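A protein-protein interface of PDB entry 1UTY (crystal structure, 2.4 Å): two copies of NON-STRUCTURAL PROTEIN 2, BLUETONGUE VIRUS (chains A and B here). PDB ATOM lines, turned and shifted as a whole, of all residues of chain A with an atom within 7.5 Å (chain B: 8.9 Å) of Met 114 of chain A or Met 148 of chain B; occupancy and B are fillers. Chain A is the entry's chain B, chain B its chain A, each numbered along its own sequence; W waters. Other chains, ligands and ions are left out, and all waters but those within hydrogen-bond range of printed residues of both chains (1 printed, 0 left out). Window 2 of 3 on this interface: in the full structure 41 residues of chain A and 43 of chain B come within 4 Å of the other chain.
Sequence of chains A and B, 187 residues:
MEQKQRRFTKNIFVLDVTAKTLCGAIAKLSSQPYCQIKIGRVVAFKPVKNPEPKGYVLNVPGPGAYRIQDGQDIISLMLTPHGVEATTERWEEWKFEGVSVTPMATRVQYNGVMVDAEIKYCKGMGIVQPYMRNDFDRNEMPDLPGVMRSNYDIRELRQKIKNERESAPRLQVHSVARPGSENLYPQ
The side-chain carboxylate (OD1) of Asp 116 of chain A lies within hydrogen-bond range of the side-chain hydroxyl (OG) of Ser 150 of chain B, at 3.4 Å.
The backbone carbonyl oxygen of Met 148 of chain B is in hydrogen-bond range of the backbone NH of Arg 107 of chain A (2.9 Å).
The side-chain hydroxyl of Ser 150 of chain B lies close to the backbone NH of Tyr 152 of chain B (3.2 Å).
O of Ala 117 of chain A lies within hydrogen-bond range of OG1 of Thr 106 of chain A (2.8 Å).
The guanidinium group (NH2) of Arg 138 of chain B lies within hydrogen-bond range of the backbone carbonyl oxygen (O) of Ser 150 of chain B (2.9 Å).
O of Pro 142 of chain B lies within hydrogen-bond range of NH2 of Arg 149 of chain B (3.0 Å).
The guanidinium group (NH1) of Arg 107 of chain A is in salt-bridge range of the side-chain carboxylate (OD2) of Asp 116 of chain A (3.7 Å).
SD of Met 114 of chain A sits close to OE1 of Gln 109 of chain A, at 3.4 Å.
Among the printed residues, pairs that only touch across the chains: Thr 106 of chain A with Met 148 of chain B (3.4 Å), Ala 105 of chain A with Tyr 152 of chain B (3.5 Å), Thr 106 of chain A with Val 147 of chain B (3.6 Å), Asn 50 of chain A with Gly 146 of chain B (3.6 Å), Ala 105 of chain A with Ser 150 of chain B (3.8 Å), Arg 107 of chain A with Arg 149 of chain B (3.9 Å), Thr 106 of chain A with Ser 150 of chain B (3.9 Å) and Met 114 of chain A with Met 148 of chain B (3.97 Å).
Met 114 of chain A touches one residue of chain B.
Met 148 of chain B touches just these residues of chain A: Thr 106 (3.4 Å), Arg 107 (2.9 Å) and Met 114 (3.97 Å).
No residue of chain B comes within 4 Å of Val 113 of chain A.
Val 115 of chain A touches none of the printed residues of chain B.
Of the printed residues of chain A, Arg 149 of chain B touches Arg 107.
Printed residues of chain B within 4 Å of Arg 107 of chain A: Met 148 and Arg 149.
Of the printed residues of chain B, Asp 116 of chain A touches Ser 150 (3.4 Å).
Printed residues of chain A within 4 Å of Ser 150 of chain B: Ala 105, Thr 106 and Asp 116.
The nearest residue of chain A that does not touch Met 148 of chain B is Ala 105 of chain A (4.7 Å).
The nearest printed residue of chain B that does not touch Arg 107 of chain A is Val 147 of chain B (4.1 Å).
Of the 14 printed residues of chain A, 6 touch a printed residue of chain B.
Of the 13 printed residues of chain B, 6 touch a printed residue of chain A.
Printed residues of chain B that touch a printed residue of chain A: Gly 146, Val 147, Met 148, Arg 149, Ser 150 and Tyr 152.
Hydrophobic or aromatic side chains of chain B that line the printed part of chain A: Val 147 and Met 148.
Among the printed residues, 10 pairs touch across the chains.
Among the printed residues, no Asp or Glu carboxylate lies within 4 Å of a Lys or Arg side-chain nitrogen of the other chain.
No position is printed for both chains.
Of the 10 pairs that touch across the chains among the printed residues, none has its exchanged pair printed and touching as well.
Water W1 lies within hydrogen-bond range of the backbone carbonyl oxygen of Gly 146 of chain B (2.6 Å) and the backbone NH of Gln 109 of chain A (2.9 Å).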
ATOM      1  N   ASN A  50      11.752  -9.675  -1.906  1.00  0.00           N
ATOM      2  CA  ASN A  50      12.627 -10.794  -2.234  1.00  0.00           C
ATOM      3  C   ASN A  50      14.005 -10.685  -1.569  1.00  0.00           C
ATOM      4  O   ASN A  50      14.441  -9.594  -1.242  1.00  0.00           O
ATOM      5  CB  ASN A  50      12.751 -10.982  -3.765  1.00  0.00           C
ATOM      6  CG  ASN A  50      13.397  -9.799  -4.451  1.00  0.00           C
ATOM      7  OD1 ASN A  50      12.716  -8.844  -4.820  1.00  0.00           O
ATOM      8  ND2 ASN A  50      14.715  -9.860  -4.643  1.00  0.00           N
ATOM      9  N   ALA A 105      20.686 -22.184  -6.257  1.00  0.00           N
ATOM     10  CA  ALA A 105      20.719 -21.381  -7.464  1.00  0.00           C
ATOM     11  C   ALA A 105      19.317 -20.834  -7.656  1.00  0.00           C
ATOM     12  O   ALA A 105      18.346 -21.590  -7.675  1.00  0.00           O
ATOM     13  CB  ALA A 105      21.145 -22.213  -8.665  1.00  0.00           C
ATOM     14  N   THR A 106      19.222 -19.511  -7.747  1.00  0.00           N
ATOM     15  CA  THR A 106      17.950 -18.827  -7.947  1.00  0.00           C
ATOM     16  C   THR A 106      18.050 -17.761  -9.036  1.00  0.00           C
ATOM     17  O   THR A 106      19.143 -17.417  -9.494  1.00  0.00           O
ATOM     18  CB  THR A 106      17.511 -18.124  -6.643  1.00  0.00           C
ATOM     19  OG1 THR A 106      18.430 -17.068  -6.348  1.00  0.00           O
ATOM     20  CG2 THR A 106      17.619 -19.044  -5.441  1.00  0.00           C
ATOM     21  N   ARG A 107      16.895 -17.235  -9.431  1.00  0.00           N
ATOM     22  CA  ARG A 107      16.829 -15.936 -10.089  1.00  0.00           C
ATOM     23  C   ARG A 107      16.108 -14.971  -9.170  1.00  0.00           C
ATOM     24  O   ARG A 107      15.043 -15.283  -8.636  1.00  0.00           O
ATOM     25  CB  ARG A 107      16.144 -16.023 -11.447  1.00  0.00           C
ATOM     26  CG  ARG A 107      17.125 -16.309 -12.561  1.00  0.00           C
ATOM     27  CD  ARG A 107      16.492 -16.653 -13.894  1.00  0.00           C
ATOM     28  NE  ARG A 107      16.041 -15.474 -14.643  1.00  0.00           N
ATOM     29  CZ  ARG A 107      16.834 -14.521 -15.137  1.00  0.00           C
ATOM     30  NH1 ARG A 107      18.150 -14.561 -14.954  1.00  0.00           N
ATOM     31  NH2 ARG A 107      16.302 -13.518 -15.823  1.00  0.00           N
ATOM     32  N   VAL A 108      16.710 -13.797  -9.009  1.00  0.00           N
ATOM     33  CA  VAL A 108      16.321 -12.810  -8.009  1.00  0.00           C
ATOM     34  C   VAL A 108      16.282 -11.387  -8.607  1.00  0.00           C
ATOM     35  O   VAL A 108      17.117 -11.042  -9.440  1.00  0.00           O
ATOM     36  CB  VAL A 108      17.318 -12.899  -6.830  1.00  0.00           C
ATOM     37  CG1 VAL A 108      17.591 -11.561  -6.215  1.00  0.00           C
ATOM     38  CG2 VAL A 108      16.827 -13.896  -5.801  1.00  0.00           C
ATOM     39  N   GLN A 109      15.307 -10.575  -8.198  1.00  0.00           N
ATOM     40  CA  GLN A 109      15.259  -9.168  -8.625  1.00  0.00           C
ATOM     41  C   GLN A 109      16.175  -8.314  -7.744  1.00  0.00           C
ATOM     42  O   GLN A 109      15.936  -8.162  -6.547  1.00  0.00           O
ATOM     43  CB  GLN A 109      13.819  -8.620  -8.658  1.00  0.00           C
ATOM     44  CG  GLN A 109      13.692  -7.120  -8.967  1.00  0.00           C
ATOM     45  CD  GLN A 109      13.092  -6.806 -10.338  1.00  0.00           C
ATOM     46  OE1 GLN A 109      13.029  -7.663 -11.229  1.00  0.00           O
ATOM     47  NE2 GLN A 109      12.666  -5.564 -10.512  1.00  0.00           N
ATOM     48  N   TYR A 110      17.223  -7.774  -8.366  1.00  0.00           N
ATOM     49  CA  TYR A 110      18.260  -6.999  -7.695  1.00  0.00           C
ATOM     50  C   TYR A 110      18.485  -5.674  -8.422  1.00  0.00           C
ATOM     51  O   TYR A 110      18.870  -5.659  -9.599  1.00  0.00           O
ATOM     52  CB  TYR A 110      19.565  -7.798  -7.655  1.00  0.00           C
ATOM     53  CG  TYR A 110      20.621  -7.229  -6.729  1.00  0.00           C
ATOM     54  CD1 TYR A 110      20.292  -6.814  -5.429  1.00  0.00           C
ATOM     55  CD2 TYR A 110      21.952  -7.117  -7.145  1.00  0.00           C
ATOM     56  CE1 TYR A 110      21.264  -6.302  -4.568  1.00  0.00           C
ATOM     57  CE2 TYR A 110      22.935  -6.607  -6.291  1.00  0.00           C
ATOM     58  CZ  TYR A 110      22.581  -6.201  -5.005  1.00  0.00           C
ATOM     59  OH  TYR A 110      23.538  -5.692  -4.156  1.00  0.00           O
ATOM     60  N   ASN A 111      18.245  -4.571  -7.710  1.00  0.00           N
ATOM     61  CA  ASN A 111      18.271  -3.224  -8.290  1.00  0.00           C
ATOM     62  C   ASN A 111      17.507  -3.128  -9.610  1.00  0.00           C
ATOM     63  O   ASN A 111      18.066  -2.726 -10.635  1.00  0.00           O
ATOM     64  CB  ASN A 111      19.711  -2.708  -8.454  1.00  0.00           C
ATOM     65  CG  ASN A 111      20.450  -2.589  -7.128  1.00  0.00           C
ATOM     66  OD1 ASN A 111      19.915  -2.074  -6.130  1.00  0.00           O
ATOM     67  ND2 ASN A 111      21.689  -3.073  -7.108  1.00  0.00           N
ATOM     68  N   GLY A 112      16.235  -3.524  -9.574  1.00  0.00           N
ATOM     69  CA  GLY A 112      15.337  -3.409 -10.715  1.00  0.00           C
ATOM     70  C   GLY A 112      15.623  -4.327 -11.896  1.00  0.00           C
ATOM     71  O   GLY A 112      15.138  -4.077 -13.004  1.00  0.00           O
ATOM     72  N   VAL A 113      16.399  -5.388 -11.662  1.00  0.00           N
ATOM     73  CA  VAL A 113      16.809  -6.309 -12.724  1.00  0.00           C
ATOM     74  C   VAL A 113      16.870  -7.760 -12.216  1.00  0.00           C
ATOM     75  O   VAL A 113      17.382  -8.018 -11.116  1.00  0.00           O
ATOM     76  CB  VAL A 113      18.167  -5.860 -13.349  1.00  0.00           C
ATOM     77  CG1 VAL A 113      18.932  -7.026 -13.970  1.00  0.00           C
ATOM     78  CG2 VAL A 113      17.944  -4.769 -14.403  1.00  0.00           C
ATOM     79  N   MET A 114      16.326  -8.686 -13.014  1.00  0.00           N
ATOM     80  CA  MET A 114      16.414 -10.125 -12.754  1.00  0.00           C
ATOM     81  C   MET A 114      17.850 -10.602 -12.915  1.00  0.00           C
ATOM     82  O   MET A 114      18.440 -10.470 -13.992  1.00  0.00           O
ATOM     83  CB  MET A 114      15.513 -10.923 -13.705  1.00  0.00           C
ATOM     84  CG  MET A 114      14.038 -10.975 -13.336  1.00  0.00           C
ATOM     85  SD  MET A 114      13.694 -11.014 -11.566  1.00  0.00           S
ATOM     86  CE  MET A 114      14.069 -12.748 -11.195  1.00  0.00           C
ATOM     87  N   VAL A 115      18.402 -11.174 -11.849  1.00  0.00           N
ATOM     88  CA  VAL A 115      19.798 -11.607 -11.854  1.00  0.00           C
ATOM     89  C   VAL A 115      19.965 -13.056 -11.360  1.00  0.00           C
ATOM     90  O   VAL A 115      19.148 -13.558 -10.584  1.00  0.00           O
ATOM     91  CB  VAL A 115      20.699 -10.580 -11.075  1.00  0.00           C
ATOM     92  CG1 VAL A 115      21.030 -11.050  -9.662  1.00  0.00           C
ATOM     93  CG2 VAL A 115      21.960 -10.249 -11.862  1.00  0.00           C
ATOM     94  N   ASP A 116      21.009 -13.729 -11.833  1.00  0.00           N
ATOM     95  CA  ASP A 116      21.331 -15.065 -11.351  1.00  0.00           C
ATOM     96  C   ASP A 116      22.081 -14.942 -10.037  1.00  0.00           C
ATOM     97  O   ASP A 116      23.065 -14.201  -9.950  1.00  0.00           O
ATOM     98  CB  ASP A 116      22.155 -15.822 -12.379  1.00  0.00           C
ATOM     99  CG  ASP A 116      21.306 -16.385 -13.492  1.00  0.00           C
ATOM    100  OD1 ASP A 116      20.353 -17.137 -13.195  1.00  0.00           O
ATOM    101  OD2 ASP A 116      21.509 -16.123 -14.692  1.00  0.00           O
ATOM    102  N   ALA A 117      21.601 -15.648  -9.012  1.00  0.00           N
ATOM    103  CA  ALA A 117      22.121 -15.455  -7.665  1.00  0.00           C
ATOM    104  C   ALA A 117      22.061 -16.702  -6.796  1.00  0.00           C
ATOM    105  O   ALA A 117      21.125 -17.509  -6.902  1.00  0.00           O
ATOM    106  CB  ALA A 117      21.390 -14.311  -6.978  1.00  0.00           C
ATOM    107  N   ARG B 138      15.099 -30.582  -7.686  1.00  0.00           N
ATOM    108  CA  ARG B 138      14.070 -29.609  -8.014  1.00  0.00           C
ATOM    109  C   ARG B 138      12.737 -29.880  -7.308  1.00  0.00           C
ATOM    110  O   ARG B 138      12.023 -28.936  -6.964  1.00  0.00           O
ATOM    111  CB  ARG B 138      13.919 -29.451  -9.531  1.00  0.00           C
ATOM    112  CG  ARG B 138      15.053 -28.638 -10.128  1.00  0.00           C
ATOM    113  CD  ARG B 138      15.161 -28.669 -11.643  1.00  0.00           C
ATOM    114  NE  ARG B 138      16.356 -27.951 -12.078  1.00  0.00           N
ATOM    115  CZ  ARG B 138      16.426 -26.633 -12.264  1.00  0.00           C
ATOM    116  NH1 ARG B 138      15.352 -25.858 -12.094  1.00  0.00           N
ATOM    117  NH2 ARG B 138      17.578 -26.091 -12.643  1.00  0.00           N
ATOM    118  N   MET B 141      12.893 -28.397  -3.553  1.00  0.00           N
ATOM    119  CA  MET B 141      13.142 -26.988  -3.299  1.00  0.00           C
ATOM    120  C   MET B 141      11.931 -26.342  -2.644  1.00  0.00           C
ATOM    121  O   MET B 141      10.787 -26.632  -3.015  1.00  0.00           O
ATOM    122  CB  MET B 141      13.515 -26.260  -4.581  1.00  0.00           C
ATOM    123  CG  MET B 141      14.917 -26.569  -5.042  1.00  0.00           C
ATOM    124  SD  MET B 141      15.362 -25.791  -6.603  1.00  0.00           S
ATOM    125  CE  MET B 141      14.149 -26.367  -7.642  1.00  0.00           C
ATOM    126  N   PRO B 142      12.189 -25.487  -1.653  1.00  0.00           N
ATOM    127  CA  PRO B 142      11.126 -24.692  -1.025  1.00  0.00           C
ATOM    128  C   PRO B 142      10.515 -23.724  -2.020  1.00  0.00           C
ATOM    129  O   PRO B 142      11.216 -23.245  -2.914  1.00  0.00           O
ATOM    130  CB  PRO B 142      11.866 -23.930   0.084  1.00  0.00           C
ATOM    131  CG  PRO B 142      13.297 -23.916  -0.345  1.00  0.00           C
ATOM    132  CD  PRO B 142      13.511 -25.224  -1.048  1.00  0.00           C
ATOM    133  N   ASP B 143       9.214 -23.483  -1.887  1.00  0.00           N
ATOM    134  CA  ASP B 143       8.556 -22.427  -2.628  1.00  0.00           C
ATOM    135  C   ASP B 143       8.750 -21.132  -1.860  1.00  0.00           C
ATOM    136  O   ASP B 143       8.154 -20.940  -0.797  1.00  0.00           O
ATOM    137  CB  ASP B 143       7.060 -22.712  -2.823  1.00  0.00           C
ATOM    138  CG  ASP B 143       6.813 -23.955  -3.650  1.00  0.00           C
ATOM    139  OD1 ASP B 143       6.834 -23.859  -4.901  1.00  0.00           O
ATOM    140  OD2 ASP B 143       6.598 -25.076  -3.136  1.00  0.00           O
ATOM    141  N   LEU B 144       9.595 -20.255  -2.394  1.00  0.00           N
ATOM    142  CA  LEU B 144       9.900 -18.993  -1.723  1.00  0.00           C
ATOM    143  C   LEU B 144       9.438 -17.787  -2.537  1.00  0.00           C
ATOM    144  O   LEU B 144       9.746 -17.688  -3.726  1.00  0.00           O
ATOM    145  CB  LEU B 144      11.396 -18.905  -1.385  1.00  0.00           C
ATOM    146  CG  LEU B 144      12.017 -20.060  -0.583  1.00  0.00           C
ATOM    147  CD1 LEU B 144      13.515 -19.868  -0.407  1.00  0.00           C
ATOM    148  CD2 LEU B 144      11.344 -20.237   0.777  1.00  0.00           C
ATOM    149  N   PRO B 145       8.690 -16.878  -1.904  1.00  0.00           N
ATOM    150  CA  PRO B 145       8.226 -15.661  -2.582  1.00  0.00           C
ATOM    151  C   PRO B 145       9.382 -14.872  -3.197  1.00  0.00           C
ATOM    152  O   PRO B 145      10.464 -14.794  -2.609  1.00  0.00           O
ATOM    153  CB  PRO B 145       7.571 -14.859  -1.454  1.00  0.00           C
ATOM    154  CG  PRO B 145       7.170 -15.871  -0.470  1.00  0.00           C
ATOM    155  CD  PRO B 145       8.237 -16.930  -0.502  1.00  0.00           C
ATOM    156  N   GLY B 146       9.144 -14.314  -4.384  1.00  0.00           N
ATOM    157  CA  GLY B 146      10.149 -13.576  -5.131  1.00  0.00           C
ATOM    158  C   GLY B 146      11.405 -14.358  -5.487  1.00  0.00           C
ATOM    159  O   GLY B 146      12.366 -13.766  -5.971  1.00  0.00           O
ATOM    160  N   VAL B 147      11.406 -15.670  -5.245  1.00  0.00           N
ATOM    161  CA  VAL B 147      12.541 -16.532  -5.585  1.00  0.00           C
ATOM    162  C   VAL B 147      12.177 -17.446  -6.757  1.00  0.00           C
ATOM    163  O   VAL B 147      11.403 -18.391  -6.616  1.00  0.00           O
ATOM    164  CB  VAL B 147      13.046 -17.363  -4.362  1.00  0.00           C
ATOM    165  CG1 VAL B 147      14.235 -18.214  -4.734  1.00  0.00           C
ATOM    166  CG2 VAL B 147      13.422 -16.441  -3.211  1.00  0.00           C
ATOM    167  N   MET B 148      12.721 -17.127  -7.925  1.00  0.00           N
ATOM    168  CA  MET B 148      12.465 -17.896  -9.137  1.00  0.00           C
ATOM    169  C   MET B 148      13.526 -18.977  -9.301  1.00  0.00           C
ATOM    170  O   MET B 148      14.594 -18.910  -8.682  1.00  0.00           O
ATOM    171  CB  MET B 148      12.445 -16.978 -10.361  1.00  0.00           C
ATOM    172  CG  MET B 148      11.047 -16.644 -10.885  1.00  0.00           C
ATOM    173  SD  MET B 148       9.981 -15.804  -9.678  1.00  0.00           S
ATOM    174  CE  MET B 148      10.681 -14.129  -9.663  1.00  0.00           C
ATOM    175  N   ARG B 149      13.215 -19.972 -10.127  1.00  0.00           N
ATOM    176  CA  ARG B 149      14.155 -21.046 -10.446  1.00  0.00           C
ATOM    177  C   ARG B 149      15.198 -20.607 -11.472  1.00  0.00           C
ATOM    178  O   ARG B 149      14.900 -19.836 -12.383  1.00  0.00           O
ATOM    179  CB  ARG B 149      13.408 -22.280 -10.960  1.00  0.00           C
ATOM    180  CG  ARG B 149      12.369 -22.844  -9.998  1.00  0.00           C
ATOM    181  CD  ARG B 149      12.941 -23.472  -8.745  1.00  0.00           C
ATOM    182  NE  ARG B 149      11.882 -23.874  -7.823  1.00  0.00           N
ATOM    183  CZ  ARG B 149      11.754 -23.441  -6.572  1.00  0.00           C
ATOM    184  NH1 ARG B 149      12.623 -22.576  -6.056  1.00  0.00           N
ATOM    185  NH2 ARG B 149      10.746 -23.880  -5.830  1.00  0.00           N
ATOM    186  N   SER B 150      16.416 -21.105 -11.294  1.00  0.00           N
ATOM    187  CA  SER B 150      17.533 -20.903 -12.207  1.00  0.00           C
ATOM    188  C   SER B 150      17.640 -22.091 -13.170  1.00  0.00           C
ATOM    189  O   SER B 150      17.237 -23.215 -12.832  1.00  0.00           O
ATOM    190  CB  SER B 150      18.834 -20.819 -11.402  1.00  0.00           C
ATOM    191  OG  SER B 150      19.914 -20.316 -12.168  1.00  0.00           O
ATOM    192  N   ASN B 151      18.191 -21.830 -14.359  1.00  0.00           N
ATOM    193  CA  ASN B 151      18.585 -22.881 -15.298  1.00  0.00           C
ATOM    194  C   ASN B 151      19.892 -23.553 -14.872  1.00  0.00           C
ATOM    195  O   ASN B 151      20.192 -24.674 -15.297  1.00  0.00           O
ATOM    196  CB  ASN B 151      18.739 -22.319 -16.722  1.00  0.00           C
ATOM    197  CG  ASN B 151      17.402 -22.019 -17.391  1.00  0.00           C
ATOM    198  OD1 ASN B 151      16.483 -22.833 -17.370  1.00  0.00           O
ATOM    199  ND2 ASN B 151      17.300 -20.849 -17.995  1.00  0.00           N
ATOM    200  N   TYR B 152      20.659 -22.866 -14.024  1.00  0.00           N
ATOM    201  CA  TYR B 152      21.960 -23.355 -13.581  1.00  0.00           C
ATOM    202  C   TYR B 152      21.884 -24.188 -12.299  1.00  0.00           C
ATOM    203  O   TYR B 152      20.895 -24.140 -11.562  1.00  0.00           O
ATOM    204  CB  TYR B 152      22.953 -22.195 -13.414  1.00  0.00           C
ATOM    205  CG  TYR B 152      23.278 -21.476 -14.712  1.00  0.00           C
ATOM    206  CD1 TYR B 152      24.270 -21.957 -15.578  1.00  0.00           C
ATOM    207  CD2 TYR B 152      22.594 -20.316 -15.079  1.00  0.00           C
ATOM    208  CE1 TYR B 152      24.567 -21.294 -16.780  1.00  0.00           C
ATOM    209  CE2 TYR B 152      22.883 -19.654 -16.268  1.00  0.00           C
ATOM    210  CZ  TYR B 152      23.868 -20.143 -17.115  1.00  0.00           C
ATOM    211  OH  TYR B 152      24.139 -19.469 -18.295  1.00  0.00           O
HETATM  212  O   HOH W   1      12.734 -11.489  -7.241  1.00  0.00           O
